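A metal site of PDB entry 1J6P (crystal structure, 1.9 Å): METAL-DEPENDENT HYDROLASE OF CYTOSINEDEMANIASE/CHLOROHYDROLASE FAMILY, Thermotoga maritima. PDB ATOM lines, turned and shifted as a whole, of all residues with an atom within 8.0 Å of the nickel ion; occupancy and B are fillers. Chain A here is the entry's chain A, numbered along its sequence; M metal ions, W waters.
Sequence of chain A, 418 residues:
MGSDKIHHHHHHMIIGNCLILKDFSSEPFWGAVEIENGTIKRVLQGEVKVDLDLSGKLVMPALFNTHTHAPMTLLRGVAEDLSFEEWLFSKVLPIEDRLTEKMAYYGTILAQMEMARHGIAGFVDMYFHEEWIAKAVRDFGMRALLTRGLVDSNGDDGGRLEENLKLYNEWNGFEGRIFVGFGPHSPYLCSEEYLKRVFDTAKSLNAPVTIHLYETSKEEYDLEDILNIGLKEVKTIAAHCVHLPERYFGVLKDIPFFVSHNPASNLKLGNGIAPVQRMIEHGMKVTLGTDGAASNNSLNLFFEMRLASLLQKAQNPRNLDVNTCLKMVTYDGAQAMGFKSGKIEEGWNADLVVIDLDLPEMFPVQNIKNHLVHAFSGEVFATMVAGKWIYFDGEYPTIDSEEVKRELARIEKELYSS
Within 4 Å of the nickel ion: His 67, His 69, His 212 and Asp 291.
Water W2 lies within hydrogen-bond range of the side-chain carboxylate of Asp 291 and a ring nitrogen (NE2) of His 240.
The nickel ion is bound by a ring nitrogen (NE2) of His 69 (2.1 Å), a ring nitrogen (NE2) of His 67 (2.1 Å), the side-chain carboxylate of Asp 291 (2.2 Å), water W2 (2.2 Å), a ring nitrogen (NE2) of His 212 (2.3 Å) and water W1 (2.3 Å).
O of Asp 291 is in hydrogen-bond range of OG1 of Thr 68. The side-chain hydroxyl (OG) of Ser 265 sits at hydrogen-bond distance from the side-chain carboxylate (OD2) of Asp 291. N of His 212 sits at hydrogen-bond distance from O of His 185, at 2.9 Å. The backbone NH of Asp 291 sits at hydrogen-bond distance from the side-chain amide oxygen of Asn 262 (2.8 Å). O of His 67 sits at hydrogen-bond distance from N of Thr 290, at 3.2 Å. O of Met 126 is in hydrogen-bond range of ND1 of His 69 (2.8 Å).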
ATOM      1  N   HIS A  67      11.389  -0.494  -4.136  1.00  0.00           N
ATOM      2  CA  HIS A  67      11.380  -0.214  -5.562  1.00  0.00           C
ATOM      3  C   HIS A  67       9.989  -0.133  -6.176  1.00  0.00           C
ATOM      4  O   HIS A  67       9.248  -1.105  -6.205  1.00  0.00           O
ATOM      5  CB  HIS A  67      12.210  -1.235  -6.360  1.00  0.00           C
ATOM      6  CG  HIS A  67      12.340  -0.892  -7.827  1.00  0.00           C
ATOM      7  ND1 HIS A  67      13.066   0.203  -8.269  1.00  0.00           N
ATOM      8  CD2 HIS A  67      11.831  -1.478  -8.941  1.00  0.00           C
ATOM      9  CE1 HIS A  67      12.999   0.277  -9.587  1.00  0.00           C
ATOM     10  NE2 HIS A  67      12.257  -0.731 -10.029  1.00  0.00           N
ATOM     11  N   THR A  68       9.629   1.029  -6.700  1.00  0.00           N
ATOM     12  CA  THR A  68       8.353   1.124  -7.412  1.00  0.00           C
ATOM     13  C   THR A  68       8.335   2.374  -8.323  1.00  0.00           C
ATOM     14  O   THR A  68       9.329   3.105  -8.385  1.00  0.00           O
ATOM     15  CB  THR A  68       7.108   1.071  -6.443  1.00  0.00           C
ATOM     16  OG1 THR A  68       5.930   0.862  -7.232  1.00  0.00           O
ATOM     17  CG2 THR A  68       6.948   2.373  -5.645  1.00  0.00           C
ATOM     18  N   HIS A  69       7.260   2.530  -9.099  1.00  0.00           N
ATOM     19  CA  HIS A  69       7.080   3.653 -10.034  1.00  0.00           C
ATOM     20  C   HIS A  69       5.599   3.903  -9.782  1.00  0.00           C
ATOM     21  O   HIS A  69       4.714   3.368 -10.478  1.00  0.00           O
ATOM     22  CB  HIS A  69       7.349   3.151 -11.471  1.00  0.00           C
ATOM     23  CG  HIS A  69       8.655   2.424 -11.585  1.00  0.00           C
ATOM     24  ND1 HIS A  69       9.870   3.077 -11.637  1.00  0.00           N
ATOM     25  CD2 HIS A  69       8.936   1.100 -11.659  1.00  0.00           C
ATOM     26  CE1 HIS A  69      10.838   2.197 -11.743  1.00  0.00           C
ATOM     27  NE2 HIS A  69      10.301   0.990 -11.760  1.00  0.00           N
ATOM     28  N   MET A  72       2.337   4.168 -12.140  1.00  0.00           N
ATOM     29  CA  MET A  72       2.062   3.065 -13.044  1.00  0.00           C
ATOM     30  C   MET A  72       0.861   2.214 -12.666  1.00  0.00           C
ATOM     31  O   MET A  72       0.484   1.273 -13.373  1.00  0.00           O
ATOM     32  CB  MET A  72       3.320   2.201 -13.283  1.00  0.00           C
ATOM     33  CG  MET A  72       4.360   3.045 -14.023  1.00  0.00           C
ATOM     34  SD  MET A  72       5.981   2.107 -14.555  1.00  0.00           S
ATOM     35  CE  MET A  72       5.291   1.461 -16.354  1.00  0.00           C
ATOM     36  N   PHE A  84      10.453  -7.947 -22.318  1.00  0.00           N
ATOM     37  CA  PHE A  84      10.838  -6.651 -21.743  1.00  0.00           C
ATOM     38  C   PHE A  84      11.011  -5.516 -22.768  1.00  0.00           C
ATOM     39  O   PHE A  84      10.524  -4.418 -22.554  1.00  0.00           O
ATOM     40  CB  PHE A  84      12.160  -6.789 -20.960  1.00  0.00           C
ATOM     41  CG  PHE A  84      12.649  -5.508 -20.371  1.00  0.00           C
ATOM     42  CD1 PHE A  84      11.849  -4.769 -19.484  1.00  0.00           C
ATOM     43  CD2 PHE A  84      13.939  -5.053 -20.654  1.00  0.00           C
ATOM     44  CE1 PHE A  84      12.326  -3.610 -18.869  1.00  0.00           C
ATOM     45  CE2 PHE A  84      14.424  -3.899 -20.044  1.00  0.00           C
ATOM     46  CZ  PHE A  84      13.628  -3.180 -19.152  1.00  0.00           C
ATOM     47  N   TRP A  87       7.566  -4.615 -23.898  1.00  0.00           N
ATOM     48  CA  TRP A  87       6.879  -3.989 -22.768  1.00  0.00           C
ATOM     49  C   TRP A  87       7.249  -2.502 -22.663  1.00  0.00           C
ATOM     50  O   TRP A  87       6.399  -1.630 -22.609  1.00  0.00           O
ATOM     51  CB  TRP A  87       7.287  -4.747 -21.467  1.00  0.00           C
ATOM     52  CG  TRP A  87       6.648  -4.287 -20.196  1.00  0.00           C
ATOM     53  CD1 TRP A  87       5.481  -4.775 -19.641  1.00  0.00           C
ATOM     54  CD2 TRP A  87       7.140  -3.296 -19.281  1.00  0.00           C
ATOM     55  NE1 TRP A  87       5.231  -4.123 -18.433  1.00  0.00           N
ATOM     56  CE2 TRP A  87       6.225  -3.216 -18.185  1.00  0.00           C
ATOM     57  CE3 TRP A  87       8.283  -2.467 -19.271  1.00  0.00           C
ATOM     58  CZ2 TRP A  87       6.415  -2.355 -17.099  1.00  0.00           C
ATOM     59  CZ3 TRP A  87       8.471  -1.584 -18.164  1.00  0.00           C
ATOM     60  CH2 TRP A  87       7.536  -1.552 -17.102  1.00  0.00           C
ATOM     61  N   MET A 126      10.944   5.826  -8.484  1.00  0.00           N
ATOM     62  CA  MET A 126      11.808   6.313  -9.554  1.00  0.00           C
ATOM     63  C   MET A 126      10.854   6.683 -10.703  1.00  0.00           C
ATOM     64  O   MET A 126      10.321   5.795 -11.397  1.00  0.00           O
ATOM     65  CB  MET A 126      12.793   5.250 -10.062  1.00  0.00           C
ATOM     66  CG  MET A 126      13.634   5.790 -11.239  1.00  0.00           C
ATOM     67  SD  MET A 126      14.300   4.199 -12.262  1.00  0.00           S
ATOM     68  CE  MET A 126      15.709   3.662 -10.980  1.00  0.00           C
ATOM     69  N   HIS A 185      18.177   5.373 -14.618  1.00  0.00           N
ATOM     70  CA  HIS A 185      17.380   4.168 -14.933  1.00  0.00           C
ATOM     71  C   HIS A 185      18.170   2.856 -14.861  1.00  0.00           C
ATOM     72  O   HIS A 185      17.708   1.849 -14.277  1.00  0.00           O
ATOM     73  CB  HIS A 185      16.720   4.316 -16.333  1.00  0.00           C
ATOM     74  CG  HIS A 185      15.960   3.097 -16.766  1.00  0.00           C
ATOM     75  ND1 HIS A 185      16.581   2.017 -17.347  1.00  0.00           N
ATOM     76  CD2 HIS A 185      14.648   2.765 -16.629  1.00  0.00           C
ATOM     77  CE1 HIS A 185      15.679   1.059 -17.545  1.00  0.00           C
ATOM     78  NE2 HIS A 185      14.504   1.493 -17.126  1.00  0.00           N
ATOM     79  N   ILE A 211      18.860   2.518  -8.846  1.00  0.00           N
ATOM     80  CA  ILE A 211      19.111   2.178 -10.246  1.00  0.00           C
ATOM     81  C   ILE A 211      18.677   0.741 -10.544  1.00  0.00           C
ATOM     82  O   ILE A 211      18.668  -0.094  -9.625  1.00  0.00           O
ATOM     83  CB  ILE A 211      20.620   2.376 -10.533  1.00  0.00           C
ATOM     84  CG1 ILE A 211      20.970   2.043 -11.990  1.00  0.00           C
ATOM     85  CG2 ILE A 211      21.463   1.499  -9.580  1.00  0.00           C
ATOM     86  CD1 ILE A 211      22.475   2.504 -12.434  1.00  0.00           C
ATOM     87  N   HIS A 212      18.256   0.445 -11.792  1.00  0.00           N
ATOM     88  CA  HIS A 212      17.880  -0.965 -12.145  1.00  0.00           C
ATOM     89  C   HIS A 212      19.236  -1.558 -12.507  1.00  0.00           C
ATOM     90  O   HIS A 212      19.867  -1.092 -13.475  1.00  0.00           O
ATOM     91  CB  HIS A 212      16.948  -1.035 -13.395  1.00  0.00           C
ATOM     92  CG  HIS A 212      15.571  -0.465 -13.195  1.00  0.00           C
ATOM     93  ND1 HIS A 212      15.096   0.599 -13.925  1.00  0.00           N
ATOM     94  CD2 HIS A 212      14.528  -0.860 -12.414  1.00  0.00           C
ATOM     95  CE1 HIS A 212      13.826   0.836 -13.613  1.00  0.00           C
ATOM     96  NE2 HIS A 212      13.458  -0.038 -12.698  1.00  0.00           N
ATOM     97  N   GLU A 215      19.262  -6.335 -14.423  1.00  0.00           N
ATOM     98  CA  GLU A 215      17.908  -6.887 -14.455  1.00  0.00           C
ATOM     99  C   GLU A 215      17.760  -7.993 -15.487  1.00  0.00           C
ATOM    100  O   GLU A 215      17.111  -8.997 -15.232  1.00  0.00           O
ATOM    101  CB  GLU A 215      16.887  -5.794 -14.794  1.00  0.00           C
ATOM    102  CG  GLU A 215      15.403  -6.289 -14.729  1.00  0.00           C
ATOM    103  CD  GLU A 215      14.416  -5.167 -14.933  1.00  0.00           C
ATOM    104  OE1 GLU A 215      14.854  -4.033 -15.290  1.00  0.00           O
ATOM    105  OE2 GLU A 215      13.201  -5.409 -14.760  1.00  0.00           O
ATOM    106  N   ALA A 239      18.039  -2.096  -7.792  1.00  0.00           N
ATOM    107  CA  ALA A 239      16.894  -3.002  -8.012  1.00  0.00           C
ATOM    108  C   ALA A 239      17.296  -4.170  -8.893  1.00  0.00           C
ATOM    109  O   ALA A 239      18.136  -4.014  -9.771  1.00  0.00           O
ATOM    110  CB  ALA A 239      15.722  -2.239  -8.686  1.00  0.00           C
ATOM    111  N   HIS A 240      16.680  -5.330  -8.636  1.00  0.00           N
ATOM    112  CA  HIS A 240      16.883  -6.582  -9.365  1.00  0.00           C
ATOM    113  C   HIS A 240      18.140  -7.389  -9.064  1.00  0.00           C
ATOM    114  O   HIS A 240      18.082  -8.354  -8.300  1.00  0.00           O
ATOM    115  CB  HIS A 240      16.730  -6.312 -10.871  1.00  0.00           C
ATOM    116  CG  HIS A 240      15.474  -5.582 -11.186  1.00  0.00           C
ATOM    117  ND1 HIS A 240      14.246  -6.003 -10.726  1.00  0.00           N
ATOM    118  CD2 HIS A 240      15.249  -4.413 -11.834  1.00  0.00           C
ATOM    119  CE1 HIS A 240      13.312  -5.135 -11.082  1.00  0.00           C
ATOM    120  NE2 HIS A 240      13.904  -4.154 -11.749  1.00  0.00           N
ATOM    121  N   ASN A 262      12.997  -7.920  -6.476  1.00  0.00           N
ATOM    122  CA  ASN A 262      11.642  -7.738  -7.036  1.00  0.00           C
ATOM    123  C   ASN A 262      11.283  -9.044  -7.707  1.00  0.00           C
ATOM    124  O   ASN A 262      11.248  -9.119  -8.945  1.00  0.00           O
ATOM    125  CB  ASN A 262      11.683  -6.654  -8.082  1.00  0.00           C
ATOM    126  CG  ASN A 262      11.757  -5.267  -7.463  1.00  0.00           C
ATOM    127  OD1 ASN A 262      10.786  -4.504  -7.512  1.00  0.00           O
ATOM    128  ND2 ASN A 262      12.884  -4.955  -6.870  1.00  0.00           N
ATOM    129  N   SER A 265       8.182  -9.190 -10.554  1.00  0.00           N
ATOM    130  CA  SER A 265       8.553  -8.506 -11.803  1.00  0.00           C
ATOM    131  C   SER A 265       9.574  -9.341 -12.582  1.00  0.00           C
ATOM    132  O   SER A 265       9.473  -9.500 -13.789  1.00  0.00           O
ATOM    133  CB  SER A 265       9.151  -7.112 -11.476  1.00  0.00           C
ATOM    134  OG  SER A 265       9.519  -6.476 -12.665  1.00  0.00           O
ATOM    135  N   LEU A 269       8.504 -10.677 -16.374  1.00  0.00           N
ATOM    136  CA  LEU A 269       9.135 -10.187 -17.577  1.00  0.00           C
ATOM    137  C   LEU A 269      10.185 -11.126 -18.129  1.00  0.00           C
ATOM    138  O   LEU A 269      10.995 -10.743 -18.985  1.00  0.00           O
ATOM    139  CB  LEU A 269       9.736  -8.767 -17.329  1.00  0.00           C
ATOM    140  CG  LEU A 269       8.693  -7.673 -17.198  1.00  0.00           C
ATOM    141  CD1 LEU A 269       9.316  -6.370 -16.685  1.00  0.00           C
ATOM    142  CD2 LEU A 269       8.036  -7.454 -18.573  1.00  0.00           C
ATOM    143  N   THR A 290       8.451  -4.031  -5.093  1.00  0.00           N
ATOM    144  CA  THR A 290       7.375  -4.589  -5.932  1.00  0.00           C
ATOM    145  C   THR A 290       7.546  -4.297  -7.414  1.00  0.00           C
ATOM    146  O   THR A 290       7.010  -5.021  -8.257  1.00  0.00           O
ATOM    147  CB  THR A 290       6.005  -3.979  -5.566  1.00  0.00           C
ATOM    148  OG1 THR A 290       6.107  -2.551  -5.637  1.00  0.00           O
ATOM    149  CG2 THR A 290       5.614  -4.356  -4.117  1.00  0.00           C
ATOM    150  N   ASP A 291       8.273  -3.211  -7.721  1.00  0.00           N
ATOM    151  CA  ASP A 291       8.396  -2.670  -9.079  1.00  0.00           C
ATOM    152  C   ASP A 291       7.050  -1.988  -9.371  1.00  0.00           C
ATOM    153  O   ASP A 291       6.274  -1.751  -8.443  1.00  0.00           O
ATOM    154  CB  ASP A 291       8.737  -3.755 -10.154  1.00  0.00           C
ATOM    155  CG  ASP A 291       9.620  -3.197 -11.278  1.00  0.00           C
ATOM    156  OD1 ASP A 291       9.801  -1.966 -11.276  1.00  0.00           O
ATOM    157  OD2 ASP A 291      10.150  -3.951 -12.129  1.00  0.00           O
ATOM    158  N   GLY A 292       6.767  -1.648 -10.624  1.00  0.00           N
ATOM    159  CA  GLY A 292       5.510  -0.950 -10.912  1.00  0.00           C
ATOM    160  C   GLY A 292       4.337  -1.875 -11.224  1.00  0.00           C
ATOM    161  O   GLY A 292       4.531  -3.057 -11.545  1.00  0.00           O
ATOM    162  N   SER A 295       4.145  -4.318 -14.329  1.00  0.00           N
ATOM    163  CA  SER A 295       4.914  -5.553 -14.402  1.00  0.00           C
ATOM    164  C   SER A 295       5.006  -6.245 -13.043  1.00  0.00           C
ATOM    165  O   SER A 295       6.083  -6.491 -12.544  1.00  0.00           O
ATOM    166  CB  SER A 295       6.341  -5.343 -14.961  1.00  0.00           C
ATOM    167  OG  SER A 295       7.157  -4.624 -14.035  1.00  0.00           O
HETATM  168 NI    NI M   1      11.426  -0.749 -12.006  1.00  0.00          NI
HETATM  169  O   HOH W   1      10.260  -0.840 -14.020  1.00  0.00           O
HETATM  170  O   HOH W   2      12.159  -2.645 -12.881  1.00  0.00           O
